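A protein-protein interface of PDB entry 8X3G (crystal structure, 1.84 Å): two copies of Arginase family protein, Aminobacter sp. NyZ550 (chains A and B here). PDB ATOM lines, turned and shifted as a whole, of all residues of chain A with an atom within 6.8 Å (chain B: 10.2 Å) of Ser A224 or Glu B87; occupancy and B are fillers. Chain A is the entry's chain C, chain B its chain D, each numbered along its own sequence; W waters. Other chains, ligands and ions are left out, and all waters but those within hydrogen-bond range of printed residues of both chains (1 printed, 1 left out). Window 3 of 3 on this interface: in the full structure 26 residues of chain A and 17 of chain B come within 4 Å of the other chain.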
ATOM      1  N   HIS A 199      11.129  24.942 -20.074  1.00  0.00           N
ATOM      2  CA  HIS A 199      12.218  25.910 -19.986  1.00  0.00           C
ATOM      3  C   HIS A 199      12.562  26.292 -21.417  1.00  0.00           C
ATOM      4  O   HIS A 199      12.900  25.414 -22.213  1.00  0.00           O
ATOM      5  CB  HIS A 199      13.445  25.332 -19.273  1.00  0.00           C
ATOM      6  CG  HIS A 199      14.520  26.356 -19.038  1.00  0.00           C
ATOM      7  ND1 HIS A 199      15.297  26.863 -20.051  1.00  0.00           N
ATOM      8  CD2 HIS A 199      14.909  26.995 -17.908  1.00  0.00           C
ATOM      9  CE1 HIS A 199      16.130  27.767 -19.555  1.00  0.00           C
ATOM     10  NE2 HIS A 199      15.931  27.847 -18.250  1.00  0.00           N
ATOM     11  N   LEU A 200      12.472  27.576 -21.744  1.00  0.00           N
ATOM     12  CA  LEU A 200      12.592  28.000 -23.138  1.00  0.00           C
ATOM     13  C   LEU A 200      13.686  29.025 -23.282  1.00  0.00           C
ATOM     14  O   LEU A 200      13.624  30.097 -22.655  1.00  0.00           O
ATOM     15  CB  LEU A 200      11.283  28.620 -23.675  1.00  0.00           C
ATOM     16  CG  LEU A 200      10.055  27.699 -23.622  1.00  0.00           C
ATOM     17  CD1 LEU A 200       9.277  27.849 -22.260  1.00  0.00           C
ATOM     18  CD2 LEU A 200       9.068  27.990 -24.801  1.00  0.00           C
ATOM     19  N   GLY A 201      14.604  28.754 -24.210  1.00  0.00           N
ATOM     20  CA  GLY A 201      15.600  29.772 -24.592  1.00  0.00           C
ATOM     21  C   GLY A 201      17.068  29.386 -24.364  1.00  0.00           C
ATOM     22  O   GLY A 201      17.948  30.223 -24.648  1.00  0.00           O
ATOM     23  N   ALA A 202      17.392  28.168 -23.888  1.00  0.00           N
ATOM     24  CA  ALA A 202      18.773  27.868 -23.486  1.00  0.00           C
ATOM     25  C   ALA A 202      19.756  28.165 -24.622  1.00  0.00           C
ATOM     26  O   ALA A 202      19.487  27.851 -25.786  1.00  0.00           O
ATOM     27  CB  ALA A 202      18.915  26.388 -23.095  1.00  0.00           C
ATOM     28  N   ARG A 203      20.906  28.775 -24.283  1.00  0.00           N
ATOM     29  CA  ARG A 203      21.870  29.214 -25.292  1.00  0.00           C
ATOM     30  C   ARG A 203      23.207  28.489 -25.184  1.00  0.00           C
ATOM     31  O   ARG A 203      23.679  28.180 -24.084  1.00  0.00           O
ATOM     32  CB  ARG A 203      22.173  30.713 -25.133  1.00  0.00           C
ATOM     33  CG  ARG A 203      20.908  31.636 -25.353  1.00  0.00           C
ATOM     34  CD  ARG A 203      20.393  31.510 -26.782  1.00  0.00           C
ATOM     35  NE  ARG A 203      21.438  31.673 -27.776  1.00  0.00           N
ATOM     36  CZ  ARG A 203      21.926  32.860 -28.145  1.00  0.00           C
ATOM     37  NH1 ARG A 203      21.470  33.982 -27.605  1.00  0.00           N
ATOM     38  NH2 ARG A 203      22.952  32.905 -29.004  1.00  0.00           N
ATOM     39  N   ASN A 204      23.868  28.300 -26.325  1.00  0.00           N
ATOM     40  CA  ASN A 204      25.250  27.865 -26.295  1.00  0.00           C
ATOM     41  C   ASN A 204      26.079  28.871 -25.491  1.00  0.00           C
ATOM     42  O   ASN A 204      25.772  30.065 -25.450  1.00  0.00           O
ATOM     43  CB  ASN A 204      25.843  27.872 -27.707  1.00  0.00           C
ATOM     44  CG  ASN A 204      25.329  26.766 -28.594  1.00  0.00           C
ATOM     45  OD1 ASN A 204      25.547  25.597 -28.289  1.00  0.00           O
ATOM     46  ND2 ASN A 204      24.676  27.141 -29.747  1.00  0.00           N
ATOM     47  N   GLN A 221      12.512  18.496 -20.384  1.00  0.00           N
ATOM     48  CA  GLN A 221      12.329  18.680 -21.830  1.00  0.00           C
ATOM     49  C   GLN A 221      12.487  20.152 -22.212  1.00  0.00           C
ATOM     50  O   GLN A 221      11.571  20.785 -22.751  1.00  0.00           O
ATOM     51  CB  GLN A 221      10.957  18.175 -22.282  1.00  0.00           C
ATOM     52  CG  GLN A 221      10.579  16.822 -21.701  1.00  0.00           C
ATOM     53  CD  GLN A 221       9.125  16.448 -21.961  1.00  0.00           C
ATOM     54  OE1 GLN A 221       8.443  15.983 -21.046  1.00  0.00           O
ATOM     55  NE2 GLN A 221       8.647  16.639 -23.206  1.00  0.00           N
ATOM     56  N   TYR A 222      13.695  20.683 -22.015  1.00  0.00           N
ATOM     57  CA  TYR A 222      13.864  22.116 -22.303  1.00  0.00           C
ATOM     58  C   TYR A 222      13.829  22.362 -23.805  1.00  0.00           C
ATOM     59  O   TYR A 222      14.137  21.465 -24.606  1.00  0.00           O
ATOM     60  CB  TYR A 222      15.187  22.657 -21.737  1.00  0.00           C
ATOM     61  CG  TYR A 222      16.402  21.949 -22.271  1.00  0.00           C
ATOM     62  CD1 TYR A 222      16.906  20.827 -21.621  1.00  0.00           C
ATOM     63  CD2 TYR A 222      17.064  22.414 -23.414  1.00  0.00           C
ATOM     64  CE1 TYR A 222      18.009  20.161 -22.089  1.00  0.00           C
ATOM     65  CE2 TYR A 222      18.208  21.751 -23.893  1.00  0.00           C
ATOM     66  CZ  TYR A 222      18.658  20.630 -23.231  1.00  0.00           C
ATOM     67  OH  TYR A 222      19.794  19.963 -23.653  1.00  0.00           O
ATOM     68  N   ASP A 223      13.362  23.559 -24.178  1.00  0.00           N
ATOM     69  CA  ASP A 223      13.319  24.044 -25.565  1.00  0.00           C
ATOM     70  C   ASP A 223      14.450  25.051 -25.732  1.00  0.00           C
ATOM     71  O   ASP A 223      14.312  26.215 -25.350  1.00  0.00           O
ATOM     72  CB  ASP A 223      11.971  24.693 -25.888  1.00  0.00           C
ATOM     73  CG  ASP A 223      10.796  23.775 -25.580  1.00  0.00           C
ATOM     74  OD1 ASP A 223      10.818  22.604 -25.991  1.00  0.00           O
ATOM     75  OD2 ASP A 223       9.875  24.198 -24.860  1.00  0.00           O
ATOM     76  N   SER A 224      15.572  24.600 -26.290  1.00  0.00           N
ATOM     77  CA  SER A 224      16.689  25.504 -26.516  1.00  0.00           C
ATOM     78  C   SER A 224      16.324  26.562 -27.568  1.00  0.00           C
ATOM     79  O   SER A 224      15.359  26.431 -28.334  1.00  0.00           O
ATOM     80  CB  SER A 224      17.909  24.694 -26.942  1.00  0.00           C
ATOM     81  OG  SER A 224      17.724  24.252 -28.286  1.00  0.00           O
ATOM     82  N   MET A 225      17.144  27.616 -27.646  1.00  0.00           N
ATOM     83  CA  MET A 225      16.899  28.627 -28.665  1.00  0.00           C
ATOM     84  C   MET A 225      16.910  28.029 -30.073  1.00  0.00           C
ATOM     85  O   MET A 225      16.044  28.346 -30.901  1.00  0.00           O
ATOM     86  CB  MET A 225      17.937  29.740 -28.515  1.00  0.00           C
ATOM     87  CG  MET A 225      17.484  31.098 -29.002  1.00  0.00           C
ATOM     88  SD  MET A 225      15.991  31.818 -28.306  1.00  0.00           S
ATOM     89  CE  MET A 225      14.913  31.731 -29.724  1.00  0.00           C
ATOM     90  N   PHE A 226      17.844  27.136 -30.343  1.00  0.00           N
ATOM     91  CA  PHE A 226      17.870  26.424 -31.621  1.00  0.00           C
ATOM     92  C   PHE A 226      16.606  25.597 -31.832  1.00  0.00           C
ATOM     93  O   PHE A 226      16.042  25.603 -32.934  1.00  0.00           O
ATOM     94  CB  PHE A 226      19.049  25.437 -31.728  1.00  0.00           C
ATOM     95  CG  PHE A 226      20.402  26.058 -31.970  1.00  0.00           C
ATOM     96  CD1 PHE A 226      20.593  27.416 -31.862  1.00  0.00           C
ATOM     97  CD2 PHE A 226      21.462  25.257 -32.421  1.00  0.00           C
ATOM     98  CE1 PHE A 226      21.862  27.956 -32.098  1.00  0.00           C
ATOM     99  CE2 PHE A 226      22.758  25.802 -32.692  1.00  0.00           C
ATOM    100  CZ  PHE A 226      22.924  27.152 -32.496  1.00  0.00           C
ATOM    101  N   ASP A 227      16.169  24.839 -30.820  1.00  0.00           N
ATOM    102  CA  ASP A 227      14.912  24.084 -30.980  1.00  0.00           C
ATOM    103  C   ASP A 227      13.780  25.015 -31.412  1.00  0.00           C
ATOM    104  O   ASP A 227      12.972  24.669 -32.294  1.00  0.00           O
ATOM    105  CB  ASP A 227      14.464  23.388 -29.682  1.00  0.00           C
ATOM    106  CG  ASP A 227      15.421  22.303 -29.190  1.00  0.00           C
ATOM    107  OD1 ASP A 227      16.065  21.626 -30.028  1.00  0.00           O
ATOM    108  OD2 ASP A 227      15.506  22.111 -27.929  1.00  0.00           O
ATOM    109  N   LEU A 228      13.697  26.182 -30.782  1.00  0.00           N
ATOM    110  CA  LEU A 228      12.633  27.146 -31.095  1.00  0.00           C
ATOM    111  C   LEU A 228      12.760  27.662 -32.518  1.00  0.00           C
ATOM    112  O   LEU A 228      11.784  27.688 -33.277  1.00  0.00           O
ATOM    113  CB  LEU A 228      12.664  28.295 -30.084  1.00  0.00           C
ATOM    114  CG  LEU A 228      12.288  27.916 -28.618  1.00  0.00           C
ATOM    115  CD1 LEU A 228      12.657  28.990 -27.660  1.00  0.00           C
ATOM    116  CD2 LEU A 228      10.788  27.552 -28.490  1.00  0.00           C
ATOM    117  N   PHE A 229      13.967  28.056 -32.919  1.00  0.00           N
ATOM    118  CA  PHE A 229      14.147  28.487 -34.301  1.00  0.00           C
ATOM    119  C   PHE A 229      13.788  27.367 -35.278  1.00  0.00           C
ATOM    120  O   PHE A 229      13.127  27.613 -36.288  1.00  0.00           O
ATOM    121  CB  PHE A 229      15.591  28.923 -34.518  1.00  0.00           C
ATOM    122  CG  PHE A 229      15.943  30.194 -33.832  1.00  0.00           C
ATOM    123  CD1 PHE A 229      15.008  31.185 -33.644  1.00  0.00           C
ATOM    124  CD2 PHE A 229      17.244  30.405 -33.393  1.00  0.00           C
ATOM    125  CE1 PHE A 229      15.339  32.373 -33.028  1.00  0.00           C
ATOM    126  CE2 PHE A 229      17.587  31.597 -32.782  1.00  0.00           C
ATOM    127  CZ  PHE A 229      16.641  32.572 -32.591  1.00  0.00           C
ATOM    128  N   ASP A 230      14.250  26.139 -35.012  1.00  0.00           N
ATOM    129  CA  ASP A 230      13.954  24.997 -35.869  1.00  0.00           C
ATOM    130  C   ASP A 230      12.465  24.784 -36.026  1.00  0.00           C
ATOM    131  O   ASP A 230      12.029  24.248 -37.048  1.00  0.00           O
ATOM    132  CB  ASP A 230      14.549  23.704 -35.325  1.00  0.00           C
ATOM    133  CG  ASP A 230      16.017  23.603 -35.552  1.00  0.00           C
ATOM    134  OD1 ASP A 230      16.497  24.292 -36.476  1.00  0.00           O
ATOM    135  OD2 ASP A 230      16.660  22.784 -34.837  1.00  0.00           O
ATOM    136  N   LEU A 236       6.345  25.081 -31.111  1.00  0.00           N
ATOM    137  CA  LEU A 236       6.996  24.473 -29.965  1.00  0.00           C
ATOM    138  C   LEU A 236       6.571  25.163 -28.677  1.00  0.00           C
ATOM    139  O   LEU A 236       6.333  24.499 -27.661  1.00  0.00           O
ATOM    140  CB  LEU A 236       8.509  24.528 -30.130  1.00  0.00           C
ATOM    141  CG  LEU A 236       9.343  23.800 -29.082  1.00  0.00           C
ATOM    142  CD1 LEU A 236       8.780  22.342 -28.733  1.00  0.00           C
ATOM    143  CD2 LEU A 236      10.826  23.710 -29.509  1.00  0.00           C
ATOM    144  N   SER B  83      33.206  27.654 -22.418  1.00  0.00           N
ATOM    145  CA  SER B  83      33.801  27.185 -23.668  1.00  0.00           C
ATOM    146  C   SER B  83      33.014  26.047 -24.314  1.00  0.00           C
ATOM    147  O   SER B  83      33.310  25.694 -25.459  1.00  0.00           O
ATOM    148  CB  SER B  83      35.276  26.759 -23.451  1.00  0.00           C
ATOM    149  OG  SER B  83      35.291  25.655 -22.581  1.00  0.00           O
ATOM    150  N   TYR B  84      32.028  25.476 -23.627  1.00  0.00           N
ATOM    151  CA  TYR B  84      31.222  24.365 -24.146  1.00  0.00           C
ATOM    152  C   TYR B  84      30.030  24.891 -24.948  1.00  0.00           C
ATOM    153  O   TYR B  84      29.271  25.746 -24.460  1.00  0.00           O
ATOM    154  CB  TYR B  84      30.729  23.479 -22.991  1.00  0.00           C
ATOM    155  CG  TYR B  84      29.898  22.290 -23.428  1.00  0.00           C
ATOM    156  CD1 TYR B  84      30.439  21.347 -24.288  1.00  0.00           C
ATOM    157  CD2 TYR B  84      28.609  22.092 -22.980  1.00  0.00           C
ATOM    158  CE1 TYR B  84      29.717  20.248 -24.695  1.00  0.00           C
ATOM    159  CE2 TYR B  84      27.871  20.969 -23.377  1.00  0.00           C
ATOM    160  CZ  TYR B  84      28.437  20.068 -24.247  1.00  0.00           C
ATOM    161  OH  TYR B  84      27.762  18.946 -24.672  1.00  0.00           O
ATOM    162  N   TRP B  85      29.843  24.338 -26.157  1.00  0.00           N
ATOM    163  CA  TRP B  85      28.798  24.707 -27.116  1.00  0.00           C
ATOM    164  C   TRP B  85      27.909  23.473 -27.206  1.00  0.00           C
ATOM    165  O   TRP B  85      28.144  22.586 -28.016  1.00  0.00           O
ATOM    166  CB  TRP B  85      29.438  25.134 -28.496  1.00  0.00           C
ATOM    167  CG  TRP B  85      29.960  26.518 -28.380  1.00  0.00           C
ATOM    168  CD1 TRP B  85      30.974  26.934 -27.589  1.00  0.00           C
ATOM    169  CD2 TRP B  85      29.384  27.704 -28.962  1.00  0.00           C
ATOM    170  NE1 TRP B  85      31.091  28.304 -27.653  1.00  0.00           N
ATOM    171  CE2 TRP B  85      30.112  28.799 -28.475  1.00  0.00           C
ATOM    172  CE3 TRP B  85      28.298  27.931 -29.825  1.00  0.00           C
ATOM    173  CZ2 TRP B  85      29.828  30.129 -28.848  1.00  0.00           C
ATOM    174  CZ3 TRP B  85      28.005  29.267 -30.211  1.00  0.00           C
ATOM    175  CH2 TRP B  85      28.795  30.340 -29.719  1.00  0.00           C
ATOM    176  N   PHE B  86      26.858  23.418 -26.369  1.00  0.00           N
ATOM    177  CA  PHE B  86      26.116  22.174 -26.265  1.00  0.00           C
ATOM    178  C   PHE B  86      25.380  21.820 -27.544  1.00  0.00           C
ATOM    179  O   PHE B  86      25.145  20.632 -27.783  1.00  0.00           O
ATOM    180  CB  PHE B  86      25.163  22.192 -25.060  1.00  0.00           C
ATOM    181  CG  PHE B  86      23.899  22.997 -25.265  1.00  0.00           C
ATOM    182  CD1 PHE B  86      22.741  22.393 -25.725  1.00  0.00           C
ATOM    183  CD2 PHE B  86      23.857  24.327 -24.924  1.00  0.00           C
ATOM    184  CE1 PHE B  86      21.533  23.144 -25.863  1.00  0.00           C
ATOM    185  CE2 PHE B  86      22.691  25.071 -25.074  1.00  0.00           C
ATOM    186  CZ  PHE B  86      21.548  24.491 -25.554  1.00  0.00           C
ATOM    187  N   GLU B  87      25.008  22.810 -28.367  1.00  0.00           N
ATOM    188  CA  GLU B  87      24.268  22.472 -29.587  1.00  0.00           C
ATOM    189  C   GLU B  87      25.166  21.777 -30.598  1.00  0.00           C
ATOM    190  O   GLU B  87      24.686  20.950 -31.386  1.00  0.00           O
ATOM    191  CB  GLU B  87      23.650  23.716 -30.220  1.00  0.00           C
ATOM    192  CG  GLU B  87      22.550  24.372 -29.362  1.00  0.00           C
ATOM    193  CD  GLU B  87      21.184  23.657 -29.355  1.00  0.00           C
ATOM    194  OE1 GLU B  87      21.027  22.485 -29.792  1.00  0.00           O
ATOM    195  OE2 GLU B  87      20.226  24.311 -28.876  1.00  0.00           O
ATOM    196  N   TYR B  88      26.469  22.053 -30.530  1.00  0.00           N
ATOM    197  CA  TYR B  88      27.454  21.433 -31.414  1.00  0.00           C
ATOM    198  C   TYR B  88      28.178  20.257 -30.756  1.00  0.00           C
ATOM    199  O   TYR B  88      28.883  19.530 -31.464  1.00  0.00           O
ATOM    200  CB  TYR B  88      28.493  22.473 -31.852  1.00  0.00           C
ATOM    201  CG  TYR B  88      27.917  23.611 -32.717  1.00  0.00           C
ATOM    202  CD1 TYR B  88      27.858  23.502 -34.102  1.00  0.00           C
ATOM    203  CD2 TYR B  88      27.470  24.782 -32.140  1.00  0.00           C
ATOM    204  CE1 TYR B  88      27.352  24.544 -34.905  1.00  0.00           C
ATOM    205  CE2 TYR B  88      26.956  25.833 -32.921  1.00  0.00           C
ATOM    206  CZ  TYR B  88      26.885  25.700 -34.285  1.00  0.00           C
ATOM    207  OH  TYR B  88      26.383  26.754 -35.002  1.00  0.00           O
ATOM    208  N   ASN B  89      27.989  20.034 -29.436  1.00  0.00           N
ATOM    209  CA  ASN B  89      28.741  19.035 -28.648  1.00  0.00           C
ATOM    210  C   ASN B  89      30.260  19.256 -28.806  1.00  0.00           C
ATOM    211  O   ASN B  89      31.044  18.317 -28.993  1.00  0.00           O
ATOM    212  CB  ASN B  89      28.354  17.605 -29.024  1.00  0.00           C
ATOM    213  CG  ASN B  89      28.917  16.553 -28.031  1.00  0.00           C
ATOM    214  OD1 ASN B  89      29.052  16.827 -26.824  1.00  0.00           O
ATOM    215  ND2 ASN B  89      29.246  15.347 -28.543  1.00  0.00           N
ATOM    216  N   VAL B  90      30.664  20.517 -28.736  1.00  0.00           N
ATOM    217  CA  VAL B  90      32.038  20.946 -28.956  1.00  0.00           C
ATOM    218  C   VAL B  90      32.488  21.711 -27.725  1.00  0.00           C
ATOM    219  O   VAL B  90      31.712  22.477 -27.151  1.00  0.00           O
ATOM    220  CB  VAL B  90      32.120  21.846 -30.223  1.00  0.00           C
ATOM    221  CG1 VAL B  90      33.382  22.685 -30.263  1.00  0.00           C
ATOM    222  CG2 VAL B  90      31.969  20.982 -31.484  1.00  0.00           C
ATOM    223  N   ASP B  91      33.746  21.540 -27.337  1.00  0.00           N
ATOM    224  CA  ASP B  91      34.320  22.358 -26.280  1.00  0.00           C
ATOM    225  C   ASP B  91      35.467  23.124 -26.917  1.00  0.00           C
ATOM    226  O   ASP B  91      36.352  22.516 -27.523  1.00  0.00           O
ATOM    227  CB  ASP B  91      34.818  21.526 -25.097  1.00  0.00           C
ATOM    228  CG  ASP B  91      35.085  22.390 -23.872  1.00  0.00           C
ATOM    229  OD1 ASP B  91      35.637  23.486 -24.013  1.00  0.00           O
ATOM    230  OD2 ASP B  91      34.702  21.992 -22.755  1.00  0.00           O
ATOM    231  N   ASP B 286      27.436  29.389 -39.920  1.00  0.00           N
ATOM    232  CA  ASP B 286      27.275  27.930 -40.151  1.00  0.00           C
ATOM    233  C   ASP B 286      27.443  27.629 -41.639  1.00  0.00           C
ATOM    234  O   ASP B 286      28.033  26.604 -41.961  1.00  0.00           O
ATOM    235  CB  ASP B 286      25.919  27.427 -39.671  1.00  0.00           C
ATOM    236  CG  ASP B 286      25.821  27.273 -38.166  1.00  0.00           C
ATOM    237  OD1 ASP B 286      26.846  26.961 -37.546  1.00  0.00           O
ATOM    238  OD2 ASP B 286      24.722  27.461 -37.635  1.00  0.00           O
ATOM    239  N   ARG B 322      31.186  31.071 -32.291  1.00  0.00           N
ATOM    240  CA  ARG B 322      30.285  30.165 -32.992  1.00  0.00           C
ATOM    241  C   ARG B 322      30.935  29.633 -34.268  1.00  0.00           C
ATOM    242  O   ARG B 322      30.729  28.471 -34.639  1.00  0.00           O
ATOM    243  CB  ARG B 322      28.984  30.895 -33.335  1.00  0.00           C
ATOM    244  CG  ARG B 322      28.026  30.058 -34.202  1.00  0.00           C
ATOM    245  CD  ARG B 322      26.670  29.892 -33.542  1.00  0.00           C
ATOM    246  NE  ARG B 322      25.720  29.268 -34.462  1.00  0.00           N
ATOM    247  CZ  ARG B 322      24.419  29.523 -34.541  1.00  0.00           C
ATOM    248  NH1 ARG B 322      23.826  30.354 -33.692  1.00  0.00           N
ATOM    249  NH2 ARG B 322      23.685  28.871 -35.451  1.00  0.00           N
ATOM    250  N   ALA B 325      33.229  26.904 -33.138  1.00  0.00           N
ATOM    251  CA  ALA B 325      32.524  25.694 -32.740  1.00  0.00           C
ATOM    252  C   ALA B 325      31.950  24.988 -33.961  1.00  0.00           C
ATOM    253  O   ALA B 325      31.943  23.750 -34.026  1.00  0.00           O
ATOM    254  CB  ALA B 325      31.402  26.052 -31.744  1.00  0.00           C
ATOM    255  N   SER B 326      31.395  25.757 -34.907  1.00  0.00           N
ATOM    256  CA  SER B 326      30.771  25.131 -36.075  1.00  0.00           C
ATOM    257  C   SER B 326      31.834  24.481 -36.964  1.00  0.00           C
ATOM    258  O   SER B 326      31.626  23.395 -37.525  1.00  0.00           O
ATOM    259  CB  SER B 326      29.956  26.196 -36.831  1.00  0.00           C
ATOM    260  OG  SER B 326      29.158  25.592 -37.849  1.00  0.00           O
ATOM    261  N   ALA B 328      34.614  23.246 -35.748  1.00  0.00           N
ATOM    262  CA  ALA B 328      34.978  22.030 -35.032  1.00  0.00           C
ATOM    263  C   ALA B 328      33.964  20.919 -35.280  1.00  0.00           C
ATOM    264  O   ALA B 328      34.344  19.765 -35.474  1.00  0.00           O
ATOM    265  CB  ALA B 328      35.095  22.301 -33.533  1.00  0.00           C
ATOM    266  N   ALA B 329      32.663  21.251 -35.284  1.00  0.00           N
ATOM    267  CA  ALA B 329      31.649  20.223 -35.538  1.00  0.00           C
ATOM    268  C   ALA B 329      31.759  19.667 -36.954  1.00  0.00           C
ATOM    269  O   ALA B 329      31.674  18.452 -37.153  1.00  0.00           O
ATOM    270  CB  ALA B 329      30.240  20.791 -35.305  1.00  0.00           C
ATOM    271  N   GLN B 330      31.951  20.548 -37.949  1.00  0.00           N
ATOM    272  CA  GLN B 330      32.161  20.102 -39.328  1.00  0.00           C
ATOM    273  C   GLN B 330      33.316  19.102 -39.421  1.00  0.00           C
ATOM    274  O   GLN B 330      33.211  18.067 -40.084  1.00  0.00           O
ATOM    275  CB  GLN B 330      32.448  21.316 -40.234  1.00  0.00           C
ATOM    276  CG  GLN B 330      32.399  20.990 -41.733  1.00  0.00           C
ATOM    277  CD  GLN B 330      31.018  20.536 -42.243  1.00  0.00           C
ATOM    278  OE1 GLN B 330      29.987  20.662 -41.556  1.00  0.00           O
ATOM    279  NE2 GLN B 330      31.016  19.957 -43.449  1.00  0.00           N
ATOM    280  N   VAL B 334      34.423  16.651 -31.794  1.00  0.00           N
ATOM    281  CA  VAL B 334      33.374  16.758 -30.779  1.00  0.00           C
ATOM    282  C   VAL B 334      33.828  16.118 -29.464  1.00  0.00           C
ATOM    283  O   VAL B 334      34.807  15.368 -29.406  1.00  0.00           O
ATOM    284  CB  VAL B 334      32.056  16.105 -31.260  1.00  0.00           C
ATOM    285  CG1 VAL B 334      31.525  16.856 -32.485  1.00  0.00           C
ATOM    286  CG2 VAL B 334      32.298  14.619 -31.574  1.00  0.00           C
ATOM    287  N   ILE B 335      33.046  16.364 -28.414  1.00  0.00           N
ATOM    288  CA  ILE B 335      33.217  15.729 -27.093  1.00  0.00           C
ATOM    289  C   ILE B 335      32.723  14.279 -27.008  1.00  0.00           C
ATOM    290  O   ILE B 335      32.288  13.694 -27.996  1.00  0.00           O
ATOM    291  CB  ILE B 335      32.510  16.571 -26.007  1.00  0.00           C
ATOM    292  CG1 ILE B 335      32.811  18.017 -26.274  1.00  0.00           C
ATOM    293  CG2 ILE B 335      32.983  16.177 -24.628  1.00  0.00           C
ATOM    294  CD1 ILE B 335      34.256  18.283 -25.950  1.00  0.00           C
HETATM  295  O   HOH W   1      20.297  27.050 -28.488  1.00  0.00           O
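The side-chain amide oxygen (OD1) of Asn A204 sits at hydrogen-bond distance from the backbone NH (N) of Phe B86, at 3.2 Å. N of Glu B87 is in hydrogen-bond range of OD1 of Asn A204. The side-chain hydroxyl of Ser A224 lies within hydrogen-bond range of the side-chain carboxylate of Glu B87 (2.6 Å).
The backbone carbonyl oxygen (O) of Ala A202 is in hydrogen-bond range of the backbone NH (N) of Met A225, 3.0 Å away. The side-chain carboxylate of Asp A227 lies within hydrogen-bond range of the backbone NH of Ser A224, 3.0 Å away. The backbone carbonyl oxygen of Val B90 lies within hydrogen-bond range of the backbone NH of Trp B85 (2.8 Å). The side-chain hydroxyl of Tyr B88 lies within hydrogen-bond range of the guanidinium group of Arg B322. The side-chain carboxylate (OD2) of Asp B286 is in salt-bridge range of the guanidinium group (NH2) of Arg B322, at 2.8 Å.
Among the printed residues, merely in contact across the chains: Asn A204 with Trp B85, Phe A226 with Glu B87, Arg A203 with Phe B86, Phe A226 with Arg B322, Ser A224 with Phe B86 and Ala A202 with Phe B86.
No residue of chain B comes within 4 Å of Gly A201. Printed residues of chain B within 4 Å of Arg A203: Phe B86 (3.4 Å). Of the printed residues of chain B, Asn A204 touches Trp B85, Phe B86 and Glu B87. Ser A224 touches two residues of chain B. No residue of chain B comes within 4 Å of Met A225. Phe A226 touches just these residues of chain B: Glu B87 (3.3 Å) and Arg B322 (3.5 Å). No residue of chain B comes within 4 Å of Asp A227. Of the printed residues of chain A, Trp B85 touches Asn A204 (3.2 Å). Of the printed residues of chain A, Phe B86 touches Ala A202, Arg A203, Asn A204 and Ser A224. Glu B87 touches just these residues of chain A: Asn A204, Ser A224 and Phe A226. Of the printed residues of chain A, Arg B322 touches Phe A226 (3.5 Å). Ala B325 touches none of the printed residues of chain A. The nearest residue of chain A that does not touch Glu B87 is Asp A227 (4.5 Å). The nearest printed residue of chain A that does not touch Trp B85 is Phe A226 (6.0 Å).
Hydrophobic or aromatic side chains of chain A that line the printed part of chain B: Phe A226. Of the 18 printed residues of chain B, 4 touch a printed residue of chain A. Among the printed residues, no Asp or Glu carboxylate lies within 4 Å of a Lys or Arg side-chain nitrogen of the other chain.
No position is printed for both chains. Of the 9 pairs that touch across the chains among the printed residues, none has its exchanged pair printed and touching as well.
Water W1 lies within hydrogen-bond range of the side-chain carboxylate of Glu B87 (2.8 Å), the backbone carbonyl oxygen of Ala A202 (2.9 Å), the backbone NH of Phe A226 (3.1 Å) and the backbone NH of Met A225 (3.3 Å).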
